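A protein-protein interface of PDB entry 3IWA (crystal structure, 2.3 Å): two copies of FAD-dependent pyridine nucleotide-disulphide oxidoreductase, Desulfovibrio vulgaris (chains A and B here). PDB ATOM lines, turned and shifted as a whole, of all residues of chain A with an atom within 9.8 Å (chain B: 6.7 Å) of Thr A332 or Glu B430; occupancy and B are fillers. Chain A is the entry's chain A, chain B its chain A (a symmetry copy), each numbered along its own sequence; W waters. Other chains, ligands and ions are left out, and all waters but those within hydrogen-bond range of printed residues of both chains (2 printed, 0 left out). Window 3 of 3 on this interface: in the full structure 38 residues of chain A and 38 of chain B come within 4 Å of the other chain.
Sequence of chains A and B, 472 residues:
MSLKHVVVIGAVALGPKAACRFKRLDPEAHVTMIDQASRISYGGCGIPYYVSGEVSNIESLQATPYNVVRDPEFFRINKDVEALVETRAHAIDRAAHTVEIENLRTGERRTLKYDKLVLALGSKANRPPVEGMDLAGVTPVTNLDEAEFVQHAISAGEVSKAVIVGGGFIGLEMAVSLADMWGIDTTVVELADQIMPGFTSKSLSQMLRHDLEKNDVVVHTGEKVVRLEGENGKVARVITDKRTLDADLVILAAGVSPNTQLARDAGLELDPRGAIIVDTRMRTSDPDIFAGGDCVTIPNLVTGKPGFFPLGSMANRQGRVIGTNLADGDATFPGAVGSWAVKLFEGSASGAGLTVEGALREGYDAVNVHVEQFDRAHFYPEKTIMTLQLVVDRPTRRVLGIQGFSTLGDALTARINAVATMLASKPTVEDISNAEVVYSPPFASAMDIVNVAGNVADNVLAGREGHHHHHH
Of chain B, only Glu B430 (2.9 Å) and Asn B434 (3.0 Å) come within 4 Å of Thr A332.
Of chain A, only Ala A331 (3.5 Å) and Thr A332 (2.9 Å) come within 4 Å of Glu B430.
No residue of chain A comes within 4 Å of Val B429.
No residue of chain A comes within 4 Å of Asp B431.
No residue of chain A comes within 4 Å of Ser B433.
Asn B434 touches just these residues of chain A: Thr A332 (3.0 Å) and Phe A333 (3.6 Å).
Of the printed residues of chain A, Asp B458 touches Arg A21 (3.6 Å) and Arg A320 (2.9 Å).
Printed residues of chain B within 4 Å of Ala A331: Glu B430.
Printed residues of chain B within 4 Å of Phe A333: Asn B434.
The nearest printed residue of chain B that does not touch Thr A332 is Asp B431 (7.1 Å).
The nearest residue of chain A that does not touch Glu B430 is Val A321 (4.2 Å).
Water W1 lies within hydrogen-bond range of OD1 of Asn B434 (2.6 Å) and O of Arg A317 (2.7 Å).
Water W2 bridges the backbone carbonyl oxygen of Asn B434 (2.8 Å) and the guanidinium group of Arg A317 (2.8 Å).
Of the 24 printed residues of chain A, 6 touch a printed residue of chain B.
Printed residues of chain A that touch a printed residue of chain B: Arg A21, Arg A317, Arg A320, Ala A331, Thr A332 and Phe A333.
Printed residues of chain B that touch a printed residue of chain A: Glu B430, Asn B434, Ala B435 and Asp B458.
Among the printed residues, 7 pairs touch across the chains.
Among the printed residues, Asp or Glu carboxylates within 4 Å of a Lys or Arg side-chain nitrogen of the other chain: Arg A21 with Asp B458 and Arg A320 with Asp B458.
No position is printed for both chains.
Of the 7 pairs that touch across the chains among the printed residues, none has its exchanged pair printed and touching as well.
Ala B435 touches Arg A317.
Ala A331 touches Glu B430 (CB to OE1, 3.5 Å).
OD1 of Asn B434 touches CD1 of Phe A333, at 3.6 Å.
The side-chain carboxylate (OE2) of Glu B430 lies within hydrogen-bond range of the side-chain hydroxyl (OG1) of Thr A332.
NH2 of Arg A21 is in salt-bridge range of OD2 of Asp B458 (3.6 Å).
The guanidinium group (NH2) of Arg A320 is in salt-bridge range of the side-chain carboxylate (OD2) of Asp B458 (2.9 Å).
The side-chain amide nitrogen (ND2) of Asn B434 sits at hydrogen-bond distance from the backbone carbonyl oxygen (O) of Thr A332, 3.0 Å away.
NE of Arg A21 sits at hydrogen-bond distance from OG1 of Thr A324, 2.6 Å away.
The guanidinium group of Arg B397 is in salt-bridge range of the side-chain carboxylate of Asp B458 (2.5 Å).
The backbone carbonyl oxygen (O) of Arg A320 is in hydrogen-bond range of the side-chain hydroxyl (OG1) of Thr A324 (3.2 Å).
The backbone carbonyl oxygen (O) of Thr A280 sits at hydrogen-bond distance from the backbone NH (N) of Phe A333 (2.8 Å).
The side-chain amide nitrogen (ND2) of Asn A325 sits at hydrogen-bond distance from the backbone carbonyl oxygen (O) of Ala A331 (2.7 Å).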
ATOM      1  N   ARG A  21     -10.931 -27.902 -23.577  1.00  0.00           N
ATOM      2  CA  ARG A  21     -10.917 -26.850 -22.557  1.00  0.00           C
ATOM      3  C   ARG A  21     -10.122 -27.316 -21.323  1.00  0.00           C
ATOM      4  O   ARG A  21      -9.358 -26.549 -20.714  1.00  0.00           O
ATOM      5  CB  ARG A  21     -12.350 -26.502 -22.156  1.00  0.00           C
ATOM      6  CG  ARG A  21     -12.498 -25.657 -20.936  1.00  0.00           C
ATOM      7  CD  ARG A  21     -11.935 -24.248 -21.106  1.00  0.00           C
ATOM      8  NE  ARG A  21     -12.218 -23.433 -19.916  1.00  0.00           N
ATOM      9  CZ  ARG A  21     -11.727 -22.217 -19.712  1.00  0.00           C
ATOM     10  NH1 ARG A  21     -10.957 -21.649 -20.620  1.00  0.00           N
ATOM     11  NH2 ARG A  21     -12.028 -21.558 -18.614  1.00  0.00           N
ATOM     12  N   ASP A 279     -26.078 -31.063 -11.255  1.00  0.00           N
ATOM     13  CA  ASP A 279     -26.133 -29.749 -10.646  1.00  0.00           C
ATOM     14  C   ASP A 279     -25.630 -28.696 -11.643  1.00  0.00           C
ATOM     15  O   ASP A 279     -25.295 -29.024 -12.795  1.00  0.00           O
ATOM     16  CB  ASP A 279     -25.363 -29.740  -9.315  1.00  0.00           C
ATOM     17  CG  ASP A 279     -23.857 -29.763  -9.480  1.00  0.00           C
ATOM     18  OD1 ASP A 279     -23.330 -29.639 -10.617  1.00  0.00           O
ATOM     19  OD2 ASP A 279     -23.187 -29.926  -8.424  1.00  0.00           O
ATOM     20  N   THR A 280     -25.537 -27.446 -11.204  1.00  0.00           N
ATOM     21  CA  THR A 280     -25.221 -26.384 -12.140  1.00  0.00           C
ATOM     22  C   THR A 280     -23.769 -26.387 -12.524  1.00  0.00           C
ATOM     23  O   THR A 280     -23.408 -25.714 -13.472  1.00  0.00           O
ATOM     24  CB  THR A 280     -25.564 -25.000 -11.602  1.00  0.00           C
ATOM     25  OG1 THR A 280     -24.750 -24.768 -10.475  1.00  0.00           O
ATOM     26  CG2 THR A 280     -27.021 -24.917 -11.205  1.00  0.00           C
ATOM     27  N   ARG A 281     -22.940 -27.143 -11.805  1.00  0.00           N
ATOM     28  CA  ARG A 281     -21.537 -27.347 -12.206  1.00  0.00           C
ATOM     29  C   ARG A 281     -21.385 -28.485 -13.237  1.00  0.00           C
ATOM     30  O   ARG A 281     -20.274 -28.804 -13.657  1.00  0.00           O
ATOM     31  CB  ARG A 281     -20.662 -27.648 -10.979  1.00  0.00           C
ATOM     32  CG  ARG A 281     -20.168 -26.455 -10.223  1.00  0.00           C
ATOM     33  CD  ARG A 281     -21.238 -25.833  -9.348  1.00  0.00           C
ATOM     34  NE  ARG A 281     -20.721 -24.639  -8.669  1.00  0.00           N
ATOM     35  CZ  ARG A 281     -21.464 -23.804  -7.929  1.00  0.00           C
ATOM     36  NH1 ARG A 281     -22.760 -24.038  -7.741  1.00  0.00           N
ATOM     37  NH2 ARG A 281     -20.912 -22.735  -7.360  1.00  0.00           N
ATOM     38  N   MET A 282     -22.526 -29.074 -13.610  1.00  0.00           N
ATOM     39  CA  MET A 282     -22.659 -30.228 -14.501  1.00  0.00           C
ATOM     40  C   MET A 282     -22.207 -31.558 -13.881  1.00  0.00           C
ATOM     41  O   MET A 282     -21.970 -32.530 -14.597  1.00  0.00           O
ATOM     42  CB  MET A 282     -22.025 -29.966 -15.876  1.00  0.00           C
ATOM     43  CG  MET A 282     -22.552 -28.686 -16.606  1.00  0.00           C
ATOM     44  SD  MET A 282     -24.340 -28.470 -16.821  1.00  0.00           S
ATOM     45  CE  MET A 282     -24.653 -29.835 -17.942  1.00  0.00           C
ATOM     46  N   ARG A 283     -22.166 -31.617 -12.551  1.00  0.00           N
ATOM     47  CA  ARG A 283     -21.864 -32.828 -11.799  1.00  0.00           C
ATOM     48  C   ARG A 283     -23.081 -33.696 -11.602  1.00  0.00           C
ATOM     49  O   ARG A 283     -24.108 -33.206 -11.171  1.00  0.00           O
ATOM     50  CB  ARG A 283     -21.352 -32.495 -10.387  1.00  0.00           C
ATOM     51  CG  ARG A 283     -19.970 -31.868 -10.332  1.00  0.00           C
ATOM     52  CD  ARG A 283     -19.395 -31.866  -8.914  1.00  0.00           C
ATOM     53  NE  ARG A 283     -17.954 -31.643  -8.983  1.00  0.00           N
ATOM     54  CZ  ARG A 283     -17.372 -30.444  -8.973  1.00  0.00           C
ATOM     55  NH1 ARG A 283     -16.048 -30.351  -9.098  1.00  0.00           N
ATOM     56  NH2 ARG A 283     -18.108 -29.342  -8.860  1.00  0.00           N
ATOM     57  N   PHE A 290     -19.095 -36.014 -14.414  1.00  0.00           N
ATOM     58  CA  PHE A 290     -19.844 -34.941 -15.056  1.00  0.00           C
ATOM     59  C   PHE A 290     -20.614 -35.547 -16.220  1.00  0.00           C
ATOM     60  O   PHE A 290     -20.233 -36.583 -16.706  1.00  0.00           O
ATOM     61  CB  PHE A 290     -18.909 -33.829 -15.597  1.00  0.00           C
ATOM     62  CG  PHE A 290     -18.054 -33.148 -14.528  1.00  0.00           C
ATOM     63  CD1 PHE A 290     -16.812 -33.675 -14.174  1.00  0.00           C
ATOM     64  CD2 PHE A 290     -18.489 -31.991 -13.908  1.00  0.00           C
ATOM     65  CE1 PHE A 290     -16.036 -33.068 -13.197  1.00  0.00           C
ATOM     66  CE2 PHE A 290     -17.736 -31.364 -12.924  1.00  0.00           C
ATOM     67  CZ  PHE A 290     -16.505 -31.888 -12.558  1.00  0.00           C
ATOM     68  N   ILE A 298     -31.679 -30.393 -17.117  1.00  0.00           N
ATOM     69  CA  ILE A 298     -31.290 -29.177 -16.412  1.00  0.00           C
ATOM     70  C   ILE A 298     -32.543 -28.306 -16.219  1.00  0.00           C
ATOM     71  O   ILE A 298     -33.529 -28.492 -16.890  1.00  0.00           O
ATOM     72  CB  ILE A 298     -30.294 -28.367 -17.202  1.00  0.00           C
ATOM     73  CG1 ILE A 298     -30.876 -28.018 -18.569  1.00  0.00           C
ATOM     74  CG2 ILE A 298     -29.011 -29.132 -17.353  1.00  0.00           C
ATOM     75  CD1 ILE A 298     -29.948 -27.264 -19.442  1.00  0.00           C
ATOM     76  N   ARG A 317     -21.480 -24.854 -24.818  1.00  0.00           N
ATOM     77  CA  ARG A 317     -21.517 -24.009 -23.641  1.00  0.00           C
ATOM     78  C   ARG A 317     -21.308 -24.885 -22.410  1.00  0.00           C
ATOM     79  O   ARG A 317     -20.494 -24.554 -21.579  1.00  0.00           O
ATOM     80  CB  ARG A 317     -22.814 -23.238 -23.570  1.00  0.00           C
ATOM     81  CG  ARG A 317     -23.027 -22.345 -24.782  1.00  0.00           C
ATOM     82  CD  ARG A 317     -24.319 -21.576 -24.733  1.00  0.00           C
ATOM     83  NE  ARG A 317     -24.561 -20.917 -26.009  1.00  0.00           N
ATOM     84  CZ  ARG A 317     -25.749 -20.744 -26.574  1.00  0.00           C
ATOM     85  NH1 ARG A 317     -26.848 -21.176 -25.981  1.00  0.00           N
ATOM     86  NH2 ARG A 317     -25.832 -20.123 -27.740  1.00  0.00           N
ATOM     87  N   GLN A 318     -22.003 -26.021 -22.351  1.00  0.00           N
ATOM     88  CA  GLN A 318     -21.898 -26.936 -21.211  1.00  0.00           C
ATOM     89  C   GLN A 318     -20.518 -27.622 -21.188  1.00  0.00           C
ATOM     90  O   GLN A 318     -19.985 -27.838 -20.144  1.00  0.00           O
ATOM     91  CB  GLN A 318     -22.996 -27.996 -21.194  1.00  0.00           C
ATOM     92  CG  GLN A 318     -24.410 -27.462 -21.129  1.00  0.00           C
ATOM     93  CD  GLN A 318     -25.450 -28.577 -21.244  1.00  0.00           C
ATOM     94  OE1 GLN A 318     -25.097 -29.749 -21.371  1.00  0.00           O
ATOM     95  NE2 GLN A 318     -26.721 -28.219 -21.151  1.00  0.00           N
ATOM     96  N   GLY A 319     -19.958 -27.904 -22.346  1.00  0.00           N
ATOM     97  CA  GLY A 319     -18.658 -28.536 -22.444  1.00  0.00           C
ATOM     98  C   GLY A 319     -17.574 -27.680 -21.842  1.00  0.00           C
ATOM     99  O   GLY A 319     -16.692 -28.188 -21.127  1.00  0.00           O
ATOM    100  N   ARG A 320     -17.646 -26.376 -22.121  1.00  0.00           N
ATOM    101  CA  ARG A 320     -16.674 -25.444 -21.605  1.00  0.00           C
ATOM    102  C   ARG A 320     -16.704 -25.460 -20.107  1.00  0.00           C
ATOM    103  O   ARG A 320     -15.672 -25.540 -19.480  1.00  0.00           O
ATOM    104  CB  ARG A 320     -16.920 -24.047 -22.121  1.00  0.00           C
ATOM    105  CG  ARG A 320     -15.828 -23.094 -21.737  1.00  0.00           C
ATOM    106  CD  ARG A 320     -16.000 -21.754 -22.463  1.00  0.00           C
ATOM    107  NE  ARG A 320     -14.741 -21.026 -22.548  1.00  0.00           N
ATOM    108  CZ  ARG A 320     -14.307 -20.149 -21.665  1.00  0.00           C
ATOM    109  NH1 ARG A 320     -13.149 -19.565 -21.881  1.00  0.00           N
ATOM    110  NH2 ARG A 320     -15.005 -19.843 -20.584  1.00  0.00           N
ATOM    111  N   VAL A 321     -17.896 -25.402 -19.533  1.00  0.00           N
ATOM    112  CA  VAL A 321     -18.045 -25.434 -18.082  1.00  0.00           C
ATOM    113  C   VAL A 321     -17.519 -26.757 -17.550  1.00  0.00           C
ATOM    114  O   VAL A 321     -16.845 -26.751 -16.524  1.00  0.00           O
ATOM    115  CB  VAL A 321     -19.516 -25.208 -17.646  1.00  0.00           C
ATOM    116  CG1 VAL A 321     -19.778 -25.605 -16.185  1.00  0.00           C
ATOM    117  CG2 VAL A 321     -19.942 -23.731 -17.921  1.00  0.00           C
ATOM    118  N   ILE A 322     -17.781 -27.883 -18.240  1.00  0.00           N
ATOM    119  CA  ILE A 322     -17.293 -29.142 -17.724  1.00  0.00           C
ATOM    120  C   ILE A 322     -15.748 -29.127 -17.771  1.00  0.00           C
ATOM    121  O   ILE A 322     -15.083 -29.496 -16.816  1.00  0.00           O
ATOM    122  CB  ILE A 322     -17.870 -30.390 -18.448  1.00  0.00           C
ATOM    123  CG1 ILE A 322     -19.376 -30.512 -18.183  1.00  0.00           C
ATOM    124  CG2 ILE A 322     -17.067 -31.647 -18.004  1.00  0.00           C
ATOM    125  CD1 ILE A 322     -20.139 -31.462 -19.116  1.00  0.00           C
ATOM    126  N   GLY A 323     -15.185 -28.638 -18.857  1.00  0.00           N
ATOM    127  CA  GLY A 323     -13.723 -28.474 -18.982  1.00  0.00           C
ATOM    128  C   GLY A 323     -13.019 -27.744 -17.847  1.00  0.00           C
ATOM    129  O   GLY A 323     -11.992 -28.195 -17.316  1.00  0.00           O
ATOM    130  N   THR A 324     -13.596 -26.614 -17.476  1.00  0.00           N
ATOM    131  CA  THR A 324     -13.121 -25.747 -16.412  1.00  0.00           C
ATOM    132  C   THR A 324     -13.263 -26.412 -15.057  1.00  0.00           C
ATOM    133  O   THR A 324     -12.366 -26.308 -14.193  1.00  0.00           O
ATOM    134  CB  THR A 324     -13.929 -24.401 -16.498  1.00  0.00           C
ATOM    135  OG1 THR A 324     -13.641 -23.785 -17.755  1.00  0.00           O
ATOM    136  CG2 THR A 324     -13.611 -23.424 -15.375  1.00  0.00           C
ATOM    137  N   ASN A 325     -14.388 -27.093 -14.843  1.00  0.00           N
ATOM    138  CA  ASN A 325     -14.605 -27.754 -13.574  1.00  0.00           C
ATOM    139  C   ASN A 325     -13.758 -29.036 -13.414  1.00  0.00           C
ATOM    140  O   ASN A 325     -13.440 -29.373 -12.305  1.00  0.00           O
ATOM    141  CB  ASN A 325     -16.097 -28.012 -13.337  1.00  0.00           C
ATOM    142  CG  ASN A 325     -16.868 -26.718 -13.172  1.00  0.00           C
ATOM    143  OD1 ASN A 325     -16.240 -25.682 -12.951  1.00  0.00           O
ATOM    144  ND2 ASN A 325     -18.221 -26.761 -13.263  1.00  0.00           N
ATOM    145  N   GLY A 329     -11.961 -25.706 -11.410  1.00  0.00           N
ATOM    146  CA  GLY A 329     -12.686 -24.412 -11.390  1.00  0.00           C
ATOM    147  C   GLY A 329     -14.058 -24.552 -10.755  1.00  0.00           C
ATOM    148  O   GLY A 329     -14.399 -25.614 -10.252  1.00  0.00           O
ATOM    149  N   ASP A 330     -14.856 -23.486 -10.799  1.00  0.00           N
ATOM    150  CA  ASP A 330     -16.216 -23.531 -10.274  1.00  0.00           C
ATOM    151  C   ASP A 330     -17.132 -22.722 -11.207  1.00  0.00           C
ATOM    152  O   ASP A 330     -17.934 -21.903 -10.782  1.00  0.00           O
ATOM    153  CB  ASP A 330     -16.234 -23.009  -8.840  1.00  0.00           C
ATOM    154  CG  ASP A 330     -17.497 -23.381  -8.081  1.00  0.00           C
ATOM    155  OD1 ASP A 330     -17.986 -24.529  -8.205  1.00  0.00           O
ATOM    156  OD2 ASP A 330     -18.000 -22.512  -7.336  1.00  0.00           O
ATOM    157  N   ALA A 331     -16.969 -22.963 -12.495  1.00  0.00           N
ATOM    158  CA  ALA A 331     -17.891 -22.481 -13.519  1.00  0.00           C
ATOM    159  C   ALA A 331     -19.288 -23.152 -13.424  1.00  0.00           C
ATOM    160  O   ALA A 331     -19.398 -24.337 -13.112  1.00  0.00           O
ATOM    161  CB  ALA A 331     -17.263 -22.701 -14.929  1.00  0.00           C
ATOM    162  N   THR A 332     -20.337 -22.362 -13.695  1.00  0.00           N
ATOM    163  CA  THR A 332     -21.728 -22.815 -13.637  1.00  0.00           C
ATOM    164  C   THR A 332     -22.514 -22.613 -14.935  1.00  0.00           C
ATOM    165  O   THR A 332     -22.228 -21.732 -15.722  1.00  0.00           O
ATOM    166  CB  THR A 332     -22.493 -22.110 -12.501  1.00  0.00           C
ATOM    167  OG1 THR A 332     -22.529 -20.701 -12.747  1.00  0.00           O
ATOM    168  CG2 THR A 332     -21.823 -22.373 -11.158  1.00  0.00           C
ATOM    169  N   PHE A 333     -23.495 -23.471 -15.142  1.00  0.00           N
ATOM    170  CA  PHE A 333     -24.439 -23.394 -16.268  1.00  0.00           C
ATOM    171  C   PHE A 333     -25.813 -23.530 -15.638  1.00  0.00           C
ATOM    172  O   PHE A 333     -26.120 -24.566 -15.047  1.00  0.00           O
ATOM    173  CB  PHE A 333     -24.187 -24.507 -17.276  1.00  0.00           C
ATOM    174  CG  PHE A 333     -24.952 -24.347 -18.527  1.00  0.00           C
ATOM    175  CD1 PHE A 333     -24.489 -23.525 -19.545  1.00  0.00           C
ATOM    176  CD2 PHE A 333     -26.176 -24.971 -18.686  1.00  0.00           C
ATOM    177  CE1 PHE A 333     -25.232 -23.363 -20.696  1.00  0.00           C
ATOM    178  CE2 PHE A 333     -26.903 -24.805 -19.821  1.00  0.00           C
ATOM    179  CZ  PHE A 333     -26.443 -24.017 -20.821  1.00  0.00           C
ATOM    180  N   PRO A 334     -26.636 -22.461 -15.698  1.00  0.00           N
ATOM    181  CA  PRO A 334     -27.840 -22.372 -14.853  1.00  0.00           C
ATOM    182  C   PRO A 334     -29.038 -23.221 -15.289  1.00  0.00           C
ATOM    183  O   PRO A 334     -29.940 -23.507 -14.485  1.00  0.00           O
ATOM    184  CB  PRO A 334     -28.218 -20.887 -14.940  1.00  0.00           C
ATOM    185  CG  PRO A 334     -27.749 -20.460 -16.337  1.00  0.00           C
ATOM    186  CD  PRO A 334     -26.427 -21.250 -16.514  1.00  0.00           C
ATOM    187  N   GLY A 335     -29.053 -23.600 -16.559  1.00  0.00           N
ATOM    188  CA  GLY A 335     -30.224 -24.222 -17.166  1.00  0.00           C
ATOM    189  C   GLY A 335     -30.438 -23.607 -18.527  1.00  0.00           C
ATOM    190  O   GLY A 335     -29.525 -23.026 -19.089  1.00  0.00           O
ATOM    191  N   ARG B 397     -15.864  -8.882 -12.707  1.00  0.00           N
ATOM    192  CA  ARG B 397     -16.164  -9.555 -13.952  1.00  0.00           C
ATOM    193  C   ARG B 397     -17.481  -9.052 -14.588  1.00  0.00           C
ATOM    194  O   ARG B 397     -18.059  -9.739 -15.397  1.00  0.00           O
ATOM    195  CB  ARG B 397     -16.189 -11.080 -13.762  1.00  0.00           C
ATOM    196  CG  ARG B 397     -14.912 -11.667 -13.200  1.00  0.00           C
ATOM    197  CD  ARG B 397     -15.049 -13.200 -12.912  1.00  0.00           C
ATOM    198  NE  ARG B 397     -15.008 -14.022 -14.129  1.00  0.00           N
ATOM    199  CZ  ARG B 397     -13.894 -14.414 -14.757  1.00  0.00           C
ATOM    200  NH1 ARG B 397     -12.674 -14.061 -14.326  1.00  0.00           N
ATOM    201  NH2 ARG B 397     -13.979 -15.162 -15.844  1.00  0.00           N
ATOM    202  N   VAL B 399     -19.923  -7.111 -17.082  1.00  0.00           N
ATOM    203  CA  VAL B 399     -19.881  -6.577 -18.432  1.00  0.00           C
ATOM    204  C   VAL B 399     -20.451  -5.170 -18.333  1.00  0.00           C
ATOM    205  O   VAL B 399     -21.482  -4.991 -17.769  1.00  0.00           O
ATOM    206  CB  VAL B 399     -20.662  -7.470 -19.412  1.00  0.00           C
ATOM    207  CG1 VAL B 399     -20.670  -6.866 -20.764  1.00  0.00           C
ATOM    208  CG2 VAL B 399     -20.031  -8.890 -19.483  1.00  0.00           C
ATOM    209  N   PRO B 427     -24.940  -8.524 -15.815  1.00  0.00           N
ATOM    210  CA  PRO B 427     -24.336  -9.780 -16.170  1.00  0.00           C
ATOM    211  C   PRO B 427     -22.818  -9.763 -15.972  1.00  0.00           C
ATOM    212  O   PRO B 427     -22.189  -8.684 -15.975  1.00  0.00           O
ATOM    213  CB  PRO B 427     -24.648  -9.876 -17.640  1.00  0.00           C
ATOM    214  CG  PRO B 427     -24.576  -8.469 -18.092  1.00  0.00           C
ATOM    215  CD  PRO B 427     -25.170  -7.677 -16.989  1.00  0.00           C
ATOM    216  N   THR B 428     -22.243 -10.955 -15.800  1.00  0.00           N
ATOM    217  CA  THR B 428     -20.813 -11.127 -15.675  1.00  0.00           C
ATOM    218  C   THR B 428     -20.388 -11.827 -16.961  1.00  0.00           C
ATOM    219  O   THR B 428     -21.227 -12.146 -17.780  1.00  0.00           O
ATOM    220  CB  THR B 428     -20.429 -12.011 -14.437  1.00  0.00           C
ATOM    221  OG1 THR B 428     -20.988 -13.332 -14.595  1.00  0.00           O
ATOM    222  CG2 THR B 428     -20.903 -11.392 -13.099  1.00  0.00           C
ATOM    223  N   VAL B 429     -19.088 -12.066 -17.117  1.00  0.00           N
ATOM    224  CA  VAL B 429     -18.513 -12.687 -18.303  1.00  0.00           C
ATOM    225  C   VAL B 429     -19.091 -14.087 -18.544  1.00  0.00           C
ATOM    226  O   VAL B 429     -19.325 -14.502 -19.689  1.00  0.00           O
ATOM    227  CB  VAL B 429     -16.993 -12.766 -18.150  1.00  0.00           C
ATOM    228  CG1 VAL B 429     -16.377 -13.756 -19.133  1.00  0.00           C
ATOM    229  CG2 VAL B 429     -16.394 -11.350 -18.308  1.00  0.00           C
ATOM    230  N   GLU B 430     -19.344 -14.799 -17.465  1.00  0.00           N
ATOM    231  CA  GLU B 430     -19.959 -16.089 -17.560  1.00  0.00           C
ATOM    232  C   GLU B 430     -21.375 -15.981 -18.193  1.00  0.00           C
ATOM    233  O   GLU B 430     -21.776 -16.861 -18.940  1.00  0.00           O
ATOM    234  CB  GLU B 430     -19.964 -16.818 -16.185  1.00  0.00           C
ATOM    235  CG  GLU B 430     -20.738 -18.151 -16.218  1.00  0.00           C
ATOM    236  CD  GLU B 430     -20.099 -19.258 -15.359  1.00  0.00           C
ATOM    237  OE1 GLU B 430     -19.365 -20.077 -15.957  1.00  0.00           O
ATOM    238  OE2 GLU B 430     -20.332 -19.291 -14.112  1.00  0.00           O
ATOM    239  N   ASP B 431     -22.111 -14.906 -17.911  1.00  0.00           N
ATOM    240  CA  ASP B 431     -23.436 -14.764 -18.466  1.00  0.00           C
ATOM    241  C   ASP B 431     -23.354 -14.557 -19.933  1.00  0.00           C
ATOM    242  O   ASP B 431     -24.266 -14.981 -20.632  1.00  0.00           O
ATOM    243  CB  ASP B 431     -24.211 -13.645 -17.834  1.00  0.00           C
ATOM    244  CG  ASP B 431     -24.569 -13.944 -16.420  1.00  0.00           C
ATOM    245  OD1 ASP B 431     -25.070 -15.048 -16.154  1.00  0.00           O
ATOM    246  OD2 ASP B 431     -24.310 -13.101 -15.562  1.00  0.00           O
ATOM    247  N   ILE B 432     -22.255 -13.969 -20.408  1.00  0.00           N
ATOM    248  CA  ILE B 432     -22.048 -13.753 -21.837  1.00  0.00           C
ATOM    249  C   ILE B 432     -21.534 -15.044 -22.512  1.00  0.00           C
ATOM    250  O   ILE B 432     -22.015 -15.419 -23.564  1.00  0.00           O
ATOM    251  CB  ILE B 432     -21.086 -12.603 -22.124  1.00  0.00           C
ATOM    252  CG1 ILE B 432     -21.534 -11.313 -21.450  1.00  0.00           C
ATOM    253  CG2 ILE B 432     -20.931 -12.400 -23.627  1.00  0.00           C
ATOM    254  CD1 ILE B 432     -22.971 -10.928 -21.619  1.00  0.00           C
ATOM    255  N   SER B 433     -20.617 -15.756 -21.865  1.00  0.00           N
ATOM    256  CA  SER B 433     -20.224 -17.123 -22.300  1.00  0.00           C
ATOM    257  C   SER B 433     -21.454 -18.043 -22.474  1.00  0.00           C
ATOM    258  O   SER B 433     -21.513 -18.846 -23.369  1.00  0.00           O
ATOM    259  CB  SER B 433     -19.228 -17.799 -21.302  1.00  0.00           C
ATOM    260  OG  SER B 433     -17.980 -17.123 -21.218  1.00  0.00           O
ATOM    261  N   ASN B 434     -22.394 -17.939 -21.567  1.00  0.00           N
ATOM    262  CA  ASN B 434     -23.584 -18.788 -21.572  1.00  0.00           C
ATOM    263  C   ASN B 434     -24.843 -18.174 -22.200  1.00  0.00           C
ATOM    264  O   ASN B 434     -25.872 -18.834 -22.201  1.00  0.00           O
ATOM    265  CB  ASN B 434     -23.903 -19.229 -20.139  1.00  0.00           C
ATOM    266  CG  ASN B 434     -22.907 -20.221 -19.612  1.00  0.00           C
ATOM    267  OD1 ASN B 434     -22.226 -20.870 -20.370  1.00  0.00           O
ATOM    268  ND2 ASN B 434     -22.825 -20.349 -18.295  1.00  0.00           N
ATOM    269  N   ALA B 435     -24.767 -16.949 -22.733  1.00  0.00           N
ATOM    270  CA  ALA B 435     -25.945 -16.234 -23.248  1.00  0.00           C
ATOM    271  C   ALA B 435     -26.664 -17.124 -24.219  1.00  0.00           C
ATOM    272  O   ALA B 435     -26.053 -17.646 -25.132  1.00  0.00           O
ATOM    273  CB  ALA B 435     -25.557 -14.930 -23.951  1.00  0.00           C
ATOM    274  N   GLY B 454     -17.428 -13.625 -24.704  1.00  0.00           N
ATOM    275  CA  GLY B 454     -17.405 -13.969 -23.277  1.00  0.00           C
ATOM    276  C   GLY B 454     -16.275 -14.942 -22.902  1.00  0.00           C
ATOM    277  O   GLY B 454     -15.681 -14.829 -21.846  1.00  0.00           O
ATOM    278  N   ASP B 458     -13.109 -14.038 -20.414  1.00  0.00           N
ATOM    279  CA  ASP B 458     -12.789 -14.897 -19.279  1.00  0.00           C
ATOM    280  C   ASP B 458     -11.313 -15.335 -19.381  1.00  0.00           C
ATOM    281  O   ASP B 458     -10.608 -15.355 -18.383  1.00  0.00           O
ATOM    282  CB  ASP B 458     -13.736 -16.099 -19.253  1.00  0.00           C
ATOM    283  CG  ASP B 458     -13.316 -17.178 -18.268  1.00  0.00           C
ATOM    284  OD1 ASP B 458     -12.805 -16.892 -17.176  1.00  0.00           O
ATOM    285  OD2 ASP B 458     -13.547 -18.335 -18.594  1.00  0.00           O
HETATM  286  O   HOH W   1     -20.047 -21.955 -21.236  1.00  0.00           O
HETATM  287  O   HOH W   2     -26.998 -21.183 -23.194  1.00  0.00           O
